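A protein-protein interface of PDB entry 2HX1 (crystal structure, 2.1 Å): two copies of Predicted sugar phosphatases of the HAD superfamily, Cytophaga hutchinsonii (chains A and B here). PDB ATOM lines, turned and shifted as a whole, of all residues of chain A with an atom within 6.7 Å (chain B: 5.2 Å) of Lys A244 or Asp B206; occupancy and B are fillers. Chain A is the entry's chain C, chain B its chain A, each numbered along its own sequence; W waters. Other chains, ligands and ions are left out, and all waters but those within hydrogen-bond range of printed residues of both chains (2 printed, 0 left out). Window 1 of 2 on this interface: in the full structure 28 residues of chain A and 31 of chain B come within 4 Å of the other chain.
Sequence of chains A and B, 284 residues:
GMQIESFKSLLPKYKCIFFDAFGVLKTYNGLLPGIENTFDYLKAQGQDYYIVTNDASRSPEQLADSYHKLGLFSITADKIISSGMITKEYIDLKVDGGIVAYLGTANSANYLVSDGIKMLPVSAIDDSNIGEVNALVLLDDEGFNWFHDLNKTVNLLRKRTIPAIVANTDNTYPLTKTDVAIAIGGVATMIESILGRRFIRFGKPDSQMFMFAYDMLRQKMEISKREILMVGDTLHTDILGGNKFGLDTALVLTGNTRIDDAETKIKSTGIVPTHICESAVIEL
OG1 of Thr A249 is in hydrogen-bond range of OD1 of Asn A243, 2.8 Å away.
Hydrophobic or aromatic side chains of chain B that line the printed part of chain A: Tyr B90, Ile B200 and Phe B202.
Printed residues of chain B within 4 Å of Leu A240: Ile B200 (3.96 Å).
Lys A244 touches five residues of chain B.
Of chain A, only Lys A244 comes within 4 Å of Asp B206.
Of the printed residues of chain A, Gln B208 touches Ser A207 (3.9 Å) and Lys A244 (2.8 Å).
The nearest residue of chain A that does not touch Asp B206 is Asp A206 (4.7 Å).
The nearest printed residue of chain B that does not touch Asn A243 is Phe B202 (6.3 Å).
The backbone carbonyl oxygen (O) of Arg B201 is in hydrogen-bond range of the side-chain amino group (NZ) of Lys A244 (3.0 Å).
The side-chain carboxylate (OD2) of Asp B206 is in salt-bridge range of the side-chain amino group (NZ) of Lys A244 (2.8 Å).
The side-chain hydroxyl of Ser B207 lies within hydrogen-bond range of the side-chain hydroxyl of Ser A207, 3.0 Å away.
The backbone carbonyl oxygen (O) of Lys A244 lies within hydrogen-bond range of the side-chain amide nitrogen (NE2) of Gln B208 (2.8 Å).
Gln B208 touches Ser A207.
Leu A240 touches Ile B200 (CD1 to CG1, 3.96 Å).
O of Asn A243 touches CE2 of Tyr B90, at 3.6 Å.
Lys A244 touches Ile B200.
CE1 of Phe B202 touches CE of Lys A244 (3.9 Å).
Water W1 bridges OD1 of Asp A206 (2.4 Å) and OD1 of Asp B206 (3.2 Å).
Water W2 lies within hydrogen-bond range of the side-chain hydroxyl (OH) of Tyr B90 (2.8 Å) and the side-chain amide nitrogen (ND2) of Asn A243 (2.9 Å).
Ser A207 touches its own counterpart, Ser B207.
Positions printed for both chains: 205, 206, 207 and 241.
Of the 9 pairs that touch across the chains among the printed residues, 1 has its exchanged pair printed and touching as well.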
ATOM      1  N   PRO A 205       6.823  -1.205  18.148  1.00  0.00           N
ATOM      2  CA  PRO A 205       6.403  -0.514  16.917  1.00  0.00           C
ATOM      3  C   PRO A 205       4.924  -0.618  16.530  1.00  0.00           C
ATOM      4  O   PRO A 205       4.567  -0.155  15.440  1.00  0.00           O
ATOM      5  CB  PRO A 205       7.264  -1.188  15.858  1.00  0.00           C
ATOM      6  CG  PRO A 205       7.234  -2.623  16.288  1.00  0.00           C
ATOM      7  CD  PRO A 205       7.348  -2.542  17.827  1.00  0.00           C
ATOM      8  N   ASP A 206       4.066  -1.138  17.412  1.00  0.00           N
ATOM      9  CA  ASP A 206       2.594  -1.097  17.180  1.00  0.00           C
ATOM     10  C   ASP A 206       2.103   0.342  17.038  1.00  0.00           C
ATOM     11  O   ASP A 206       2.649   1.236  17.635  1.00  0.00           O
ATOM     12  CB  ASP A 206       1.781  -1.756  18.318  1.00  0.00           C
ATOM     13  CG  ASP A 206       2.057  -3.267  18.488  1.00  0.00           C
ATOM     14  OD1 ASP A 206       2.668  -3.874  17.586  1.00  0.00           O
ATOM     15  OD2 ASP A 206       1.650  -3.840  19.535  1.00  0.00           O
ATOM     16  N   SER A 207       1.015   0.527  16.302  1.00  0.00           N
ATOM     17  CA  SER A 207       0.460   1.851  15.995  1.00  0.00           C
ATOM     18  C   SER A 207      -0.485   2.383  17.070  1.00  0.00           C
ATOM     19  O   SER A 207      -0.878   3.541  17.018  1.00  0.00           O
ATOM     20  CB  SER A 207      -0.296   1.825  14.655  1.00  0.00           C
ATOM     21  OG  SER A 207      -1.491   1.042  14.711  1.00  0.00           O
ATOM     22  N   LYS A 225      -0.721  13.614   9.395  1.00  0.00           N
ATOM     23  CA  LYS A 225       0.429  12.772   9.737  1.00  0.00           C
ATOM     24  C   LYS A 225       1.729  13.381   9.251  1.00  0.00           C
ATOM     25  O   LYS A 225       2.791  13.052   9.779  1.00  0.00           O
ATOM     26  CB  LYS A 225       0.269  11.379   9.168  1.00  0.00           C
ATOM     27  CG  LYS A 225      -0.796  10.571   9.869  1.00  0.00           C
ATOM     28  CD  LYS A 225      -0.838   9.169   9.330  1.00  0.00           C
ATOM     29  CE  LYS A 225      -1.701   8.271  10.169  1.00  0.00           C
ATOM     30  NZ  LYS A 225      -1.686   6.902   9.593  1.00  0.00           N
ATOM     31  N   ILE A 239      11.717   3.931  15.039  1.00  0.00           N
ATOM     32  CA  ILE A 239      11.773   4.349  13.658  1.00  0.00           C
ATOM     33  C   ILE A 239      10.808   3.514  12.840  1.00  0.00           C
ATOM     34  O   ILE A 239      10.003   4.071  12.081  1.00  0.00           O
ATOM     35  CB  ILE A 239      13.197   4.347  13.087  1.00  0.00           C
ATOM     36  CG1 ILE A 239      14.123   5.199  13.958  1.00  0.00           C
ATOM     37  CG2 ILE A 239      13.211   4.906  11.643  1.00  0.00           C
ATOM     38  CD1 ILE A 239      13.588   6.632  14.250  1.00  0.00           C
ATOM     39  N   LEU A 240      10.853   2.193  13.022  1.00  0.00           N
ATOM     40  CA  LEU A 240       9.987   1.291  12.279  1.00  0.00           C
ATOM     41  C   LEU A 240       8.532   1.602  12.555  1.00  0.00           C
ATOM     42  O   LEU A 240       7.710   1.686  11.637  1.00  0.00           O
ATOM     43  CB  LEU A 240      10.284  -0.170  12.614  1.00  0.00           C
ATOM     44  CG  LEU A 240       9.352  -1.263  12.044  1.00  0.00           C
ATOM     45  CD1 LEU A 240       9.143  -1.226  10.530  1.00  0.00           C
ATOM     46  CD2 LEU A 240       9.926  -2.606  12.487  1.00  0.00           C
ATOM     47  N   GLY A 241       8.216   1.816  13.821  1.00  0.00           N
ATOM     48  CA  GLY A 241       6.828   2.066  14.206  1.00  0.00           C
ATOM     49  C   GLY A 241       6.322   3.358  13.618  1.00  0.00           C
ATOM     50  O   GLY A 241       5.213   3.417  13.047  1.00  0.00           O
ATOM     51  N   GLY A 242       7.115   4.414  13.760  1.00  0.00           N
ATOM     52  CA  GLY A 242       6.734   5.680  13.169  1.00  0.00           C
ATOM     53  C   GLY A 242       6.545   5.594  11.662  1.00  0.00           C
ATOM     54  O   GLY A 242       5.548   6.139  11.092  1.00  0.00           O
ATOM     55  N   ASN A 243       7.492   4.936  10.999  1.00  0.00           N
ATOM     56  CA  ASN A 243       7.417   4.815   9.539  1.00  0.00           C
ATOM     57  C   ASN A 243       6.130   4.099   9.156  1.00  0.00           C
ATOM     58  O   ASN A 243       5.352   4.620   8.340  1.00  0.00           O
ATOM     59  CB  ASN A 243       8.652   4.123   8.928  1.00  0.00           C
ATOM     60  CG  ASN A 243       9.882   5.049   8.861  1.00  0.00           C
ATOM     61  OD1 ASN A 243       9.773   6.279   9.037  1.00  0.00           O
ATOM     62  ND2 ASN A 243      11.061   4.460   8.609  1.00  0.00           N
ATOM     63  N   LYS A 244       5.886   2.928   9.732  1.00  0.00           N
ATOM     64  CA  LYS A 244       4.670   2.162   9.367  1.00  0.00           C
ATOM     65  C   LYS A 244       3.379   2.947   9.571  1.00  0.00           C
ATOM     66  O   LYS A 244       2.397   2.714   8.859  1.00  0.00           O
ATOM     67  CB  LYS A 244       4.536   0.837  10.134  1.00  0.00           C
ATOM     68  CG  LYS A 244       5.583  -0.187   9.797  1.00  0.00           C
ATOM     69  CD  LYS A 244       5.451  -1.426  10.673  1.00  0.00           C
ATOM     70  CE  LYS A 244       4.354  -2.391  10.175  1.00  0.00           C
ATOM     71  NZ  LYS A 244       4.148  -3.556  11.133  1.00  0.00           N
ATOM     72  N   PHE A 245       3.360   3.860  10.537  1.00  0.00           N
ATOM     73  CA  PHE A 245       2.153   4.618  10.824  1.00  0.00           C
ATOM     74  C   PHE A 245       2.022   5.842   9.894  1.00  0.00           C
ATOM     75  O   PHE A 245       1.024   6.558   9.941  1.00  0.00           O
ATOM     76  CB  PHE A 245       2.135   5.015  12.318  1.00  0.00           C
ATOM     77  CG  PHE A 245       0.841   5.650  12.777  1.00  0.00           C
ATOM     78  CD1 PHE A 245      -0.325   4.904  12.844  1.00  0.00           C
ATOM     79  CD2 PHE A 245       0.790   6.983  13.146  1.00  0.00           C
ATOM     80  CE1 PHE A 245      -1.526   5.486  13.267  1.00  0.00           C
ATOM     81  CE2 PHE A 245      -0.409   7.575  13.566  1.00  0.00           C
ATOM     82  CZ  PHE A 245      -1.562   6.824  13.624  1.00  0.00           C
ATOM     83  N   GLY A 246       3.016   6.088   9.042  1.00  0.00           N
ATOM     84  CA  GLY A 246       2.952   7.227   8.134  1.00  0.00           C
ATOM     85  C   GLY A 246       3.608   8.506   8.649  1.00  0.00           C
ATOM     86  O   GLY A 246       3.481   9.570   8.032  1.00  0.00           O
ATOM     87  N   LEU A 247       4.373   8.420   9.731  1.00  0.00           N
ATOM     88  CA  LEU A 247       5.056   9.612  10.242  1.00  0.00           C
ATOM     89  C   LEU A 247       6.464   9.751   9.706  1.00  0.00           C
ATOM     90  O   LEU A 247       7.158   8.761   9.479  1.00  0.00           O
ATOM     91  CB  LEU A 247       5.114   9.575  11.769  1.00  0.00           C
ATOM     92  CG  LEU A 247       3.852   9.159  12.522  1.00  0.00           C
ATOM     93  CD1 LEU A 247       4.185   9.106  14.043  1.00  0.00           C
ATOM     94  CD2 LEU A 247       2.643  10.086  12.228  1.00  0.00           C
ATOM     95  N   THR A 249      10.185  10.255  10.537  1.00  0.00           N
ATOM     96  CA  THR A 249      10.986   9.817  11.672  1.00  0.00           C
ATOM     97  C   THR A 249      12.369  10.484  11.718  1.00  0.00           C
ATOM     98  O   THR A 249      12.997  10.785  10.685  1.00  0.00           O
ATOM     99  CB  THR A 249      11.111   8.300  11.668  1.00  0.00           C
ATOM    100  OG1 THR A 249      11.595   7.854  10.400  1.00  0.00           O
ATOM    101  CG2 THR A 249       9.730   7.649  11.927  1.00  0.00           C
ATOM    102  N   ILE B  86      -2.496  -0.583   2.751  1.00  0.00           N
ATOM    103  CA  ILE B  86      -1.463  -0.035   3.592  1.00  0.00           C
ATOM    104  C   ILE B  86      -0.170   0.071   2.806  1.00  0.00           C
ATOM    105  O   ILE B  86       0.517   1.103   2.844  1.00  0.00           O
ATOM    106  CB  ILE B  86      -1.172  -0.887   4.843  1.00  0.00           C
ATOM    107  CG1 ILE B  86      -2.426  -1.096   5.696  1.00  0.00           C
ATOM    108  CG2 ILE B  86      -0.072  -0.203   5.669  1.00  0.00           C
ATOM    109  CD1 ILE B  86      -2.226  -2.121   6.790  1.00  0.00           C
ATOM    110  N   TYR B  90       2.049   3.368   1.946  1.00  0.00           N
ATOM    111  CA  TYR B  90       3.435   3.406   2.402  1.00  0.00           C
ATOM    112  C   TYR B  90       4.382   3.755   1.272  1.00  0.00           C
ATOM    113  O   TYR B  90       5.254   4.589   1.451  1.00  0.00           O
ATOM    114  CB  TYR B  90       3.857   2.087   3.047  1.00  0.00           C
ATOM    115  CG  TYR B  90       5.206   2.165   3.732  1.00  0.00           C
ATOM    116  CD1 TYR B  90       6.393   1.993   3.015  1.00  0.00           C
ATOM    117  CD2 TYR B  90       5.295   2.412   5.090  1.00  0.00           C
ATOM    118  CE1 TYR B  90       7.645   2.065   3.642  1.00  0.00           C
ATOM    119  CE2 TYR B  90       6.535   2.523   5.717  1.00  0.00           C
ATOM    120  CZ  TYR B  90       7.699   2.340   4.986  1.00  0.00           C
ATOM    121  OH  TYR B  90       8.916   2.400   5.615  1.00  0.00           O
ATOM    122  N   ILE B 200       9.210  -5.414   6.477  1.00  0.00           N
ATOM    123  CA  ILE B 200       8.082  -4.694   7.054  1.00  0.00           C
ATOM    124  C   ILE B 200       6.848  -5.484   6.664  1.00  0.00           C
ATOM    125  O   ILE B 200       6.582  -5.702   5.467  1.00  0.00           O
ATOM    126  CB  ILE B 200       7.922  -3.270   6.478  1.00  0.00           C
ATOM    127  CG1 ILE B 200       9.172  -2.400   6.751  1.00  0.00           C
ATOM    128  CG2 ILE B 200       6.681  -2.606   7.116  1.00  0.00           C
ATOM    129  CD1 ILE B 200       9.541  -1.425   5.636  1.00  0.00           C
ATOM    130  N   ARG B 201       6.113  -5.933   7.668  1.00  0.00           N
ATOM    131  CA  ARG B 201       4.910  -6.719   7.452  1.00  0.00           C
ATOM    132  C   ARG B 201       3.647  -5.914   7.778  1.00  0.00           C
ATOM    133  O   ARG B 201       3.541  -5.359   8.848  1.00  0.00           O
ATOM    134  CB  ARG B 201       4.983  -7.959   8.337  1.00  0.00           C
ATOM    135  CG  ARG B 201       5.950  -9.029   7.761  1.00  0.00           C
ATOM    136  CD  ARG B 201       6.226 -10.135   8.732  1.00  0.00           C
ATOM    137  NE  ARG B 201       7.127 -11.128   8.139  1.00  0.00           N
ATOM    138  CZ  ARG B 201       6.748 -12.252   7.528  1.00  0.00           C
ATOM    139  NH1 ARG B 201       5.460 -12.573   7.403  1.00  0.00           N
ATOM    140  NH2 ARG B 201       7.674 -13.074   7.033  1.00  0.00           N
ATOM    141  N   PHE B 202       2.701  -5.867   6.849  1.00  0.00           N
ATOM    142  CA  PHE B 202       1.459  -5.105   7.027  1.00  0.00           C
ATOM    143  C   PHE B 202       0.306  -6.053   7.169  1.00  0.00           C
ATOM    144  O   PHE B 202       0.270  -7.120   6.524  1.00  0.00           O
ATOM    145  CB  PHE B 202       1.200  -4.187   5.832  1.00  0.00           C
ATOM    146  CG  PHE B 202       2.181  -3.013   5.725  1.00  0.00           C
ATOM    147  CD1 PHE B 202       2.388  -2.160   6.800  1.00  0.00           C
ATOM    148  CD2 PHE B 202       2.847  -2.760   4.544  1.00  0.00           C
ATOM    149  CE1 PHE B 202       3.253  -1.066   6.701  1.00  0.00           C
ATOM    150  CE2 PHE B 202       3.713  -1.669   4.436  1.00  0.00           C
ATOM    151  CZ  PHE B 202       3.912  -0.832   5.518  1.00  0.00           C
ATOM    152  N   GLY B 203      -0.629  -5.663   8.023  1.00  0.00           N
ATOM    153  CA  GLY B 203      -1.868  -6.395   8.198  1.00  0.00           C
ATOM    154  C   GLY B 203      -1.944  -6.981   9.571  1.00  0.00           C
ATOM    155  O   GLY B 203      -1.049  -6.781  10.403  1.00  0.00           O
ATOM    156  N   LYS B 204      -3.009  -7.759   9.781  1.00  0.00           N
ATOM    157  CA  LYS B 204      -3.266  -8.412  11.058  1.00  0.00           C
ATOM    158  C   LYS B 204      -2.027  -9.214  11.440  1.00  0.00           C
ATOM    159  O   LYS B 204      -1.445  -9.861  10.579  1.00  0.00           O
ATOM    160  CB  LYS B 204      -4.489  -9.344  10.957  1.00  0.00           C
ATOM    161  CG  LYS B 204      -5.781  -8.681  10.381  1.00  0.00           C
ATOM    162  CD  LYS B 204      -6.863  -9.714  10.105  1.00  0.00           C
ATOM    163  CE  LYS B 204      -6.576 -10.559   8.865  1.00  0.00           C
ATOM    164  NZ  LYS B 204      -7.747 -11.354   8.468  1.00  0.00           N
ATOM    165  N   PRO B 205      -1.656  -9.217  12.731  1.00  0.00           N
ATOM    166  CA  PRO B 205      -2.317  -8.681  13.927  1.00  0.00           C
ATOM    167  C   PRO B 205      -2.093  -7.185  14.256  1.00  0.00           C
ATOM    168  O   PRO B 205      -2.453  -6.738  15.365  1.00  0.00           O
ATOM    169  CB  PRO B 205      -1.696  -9.514  15.034  1.00  0.00           C
ATOM    170  CG  PRO B 205      -0.294  -9.726  14.570  1.00  0.00           C
ATOM    171  CD  PRO B 205      -0.407  -9.917  13.071  1.00  0.00           C
ATOM    172  N   ASP B 206      -1.520  -6.420  13.323  1.00  0.00           N
ATOM    173  CA  ASP B 206      -1.451  -4.954  13.463  1.00  0.00           C
ATOM    174  C   ASP B 206      -2.891  -4.449  13.449  1.00  0.00           C
ATOM    175  O   ASP B 206      -3.808  -5.210  13.133  1.00  0.00           O
ATOM    176  CB  ASP B 206      -0.706  -4.285  12.299  1.00  0.00           C
ATOM    177  CG  ASP B 206       0.812  -4.593  12.267  1.00  0.00           C
ATOM    178  OD1 ASP B 206       1.378  -5.180  13.246  1.00  0.00           O
ATOM    179  OD2 ASP B 206       1.431  -4.195  11.240  1.00  0.00           O
ATOM    180  N   SER B 207      -3.067  -3.164  13.766  1.00  0.00           N
ATOM    181  CA  SER B 207      -4.380  -2.585  14.026  1.00  0.00           C
ATOM    182  C   SER B 207      -4.782  -1.452  13.080  1.00  0.00           C
ATOM    183  O   SER B 207      -5.860  -0.853  13.277  1.00  0.00           O
ATOM    184  CB  SER B 207      -4.423  -2.069  15.451  1.00  0.00           C
ATOM    185  OG  SER B 207      -3.601  -0.928  15.591  1.00  0.00           O
ATOM    186  N   GLN B 208      -3.951  -1.150  12.067  1.00  0.00           N
ATOM    187  CA  GLN B 208      -4.257  -0.033  11.159  1.00  0.00           C
ATOM    188  C   GLN B 208      -5.537  -0.242  10.397  1.00  0.00           C
ATOM    189  O   GLN B 208      -6.317   0.688  10.255  1.00  0.00           O
ATOM    190  CB  GLN B 208      -3.112   0.293  10.174  1.00  0.00           C
ATOM    191  CG  GLN B 208      -1.832   0.846  10.853  1.00  0.00           C
ATOM    192  CD  GLN B 208      -0.880   1.568   9.884  1.00  0.00           C
ATOM    193  OE1 GLN B 208      -1.198   2.642   9.390  1.00  0.00           O
ATOM    194  NE2 GLN B 208       0.293   0.976   9.622  1.00  0.00           N
ATOM    195  N   PHE B 210      -8.139  -2.157  11.170  1.00  0.00           N
ATOM    196  CA  PHE B 210      -9.208  -2.079  12.161  1.00  0.00           C
ATOM    197  C   PHE B 210      -9.522  -0.626  12.434  1.00  0.00           C
ATOM    198  O   PHE B 210     -10.667  -0.237  12.471  1.00  0.00           O
ATOM    199  CB  PHE B 210      -8.813  -2.719  13.502  1.00  0.00           C
ATOM    200  CG  PHE B 210      -8.552  -4.212  13.455  1.00  0.00           C
ATOM    201  CD1 PHE B 210      -9.212  -5.046  12.579  1.00  0.00           C
ATOM    202  CD2 PHE B 210      -7.636  -4.775  14.331  1.00  0.00           C
ATOM    203  CE1 PHE B 210      -8.961  -6.425  12.579  1.00  0.00           C
ATOM    204  CE2 PHE B 210      -7.370  -6.125  14.328  1.00  0.00           C
ATOM    205  CZ  PHE B 210      -8.039  -6.964  13.451  1.00  0.00           C
ATOM    206  N   GLY B 241      -4.857 -10.119  16.903  1.00  0.00           N
ATOM    207  CA  GLY B 241      -5.005  -8.784  16.344  1.00  0.00           C
ATOM    208  C   GLY B 241      -6.233  -8.084  16.866  1.00  0.00           C
ATOM    209  O   GLY B 241      -6.147  -6.982  17.380  1.00  0.00           O
HETATM  210  O   HOH W   1       3.565  -4.097  15.320  1.00  0.00           O
HETATM  211  O   HOH W   2      10.522   1.723   7.840  1.00  0.00           O
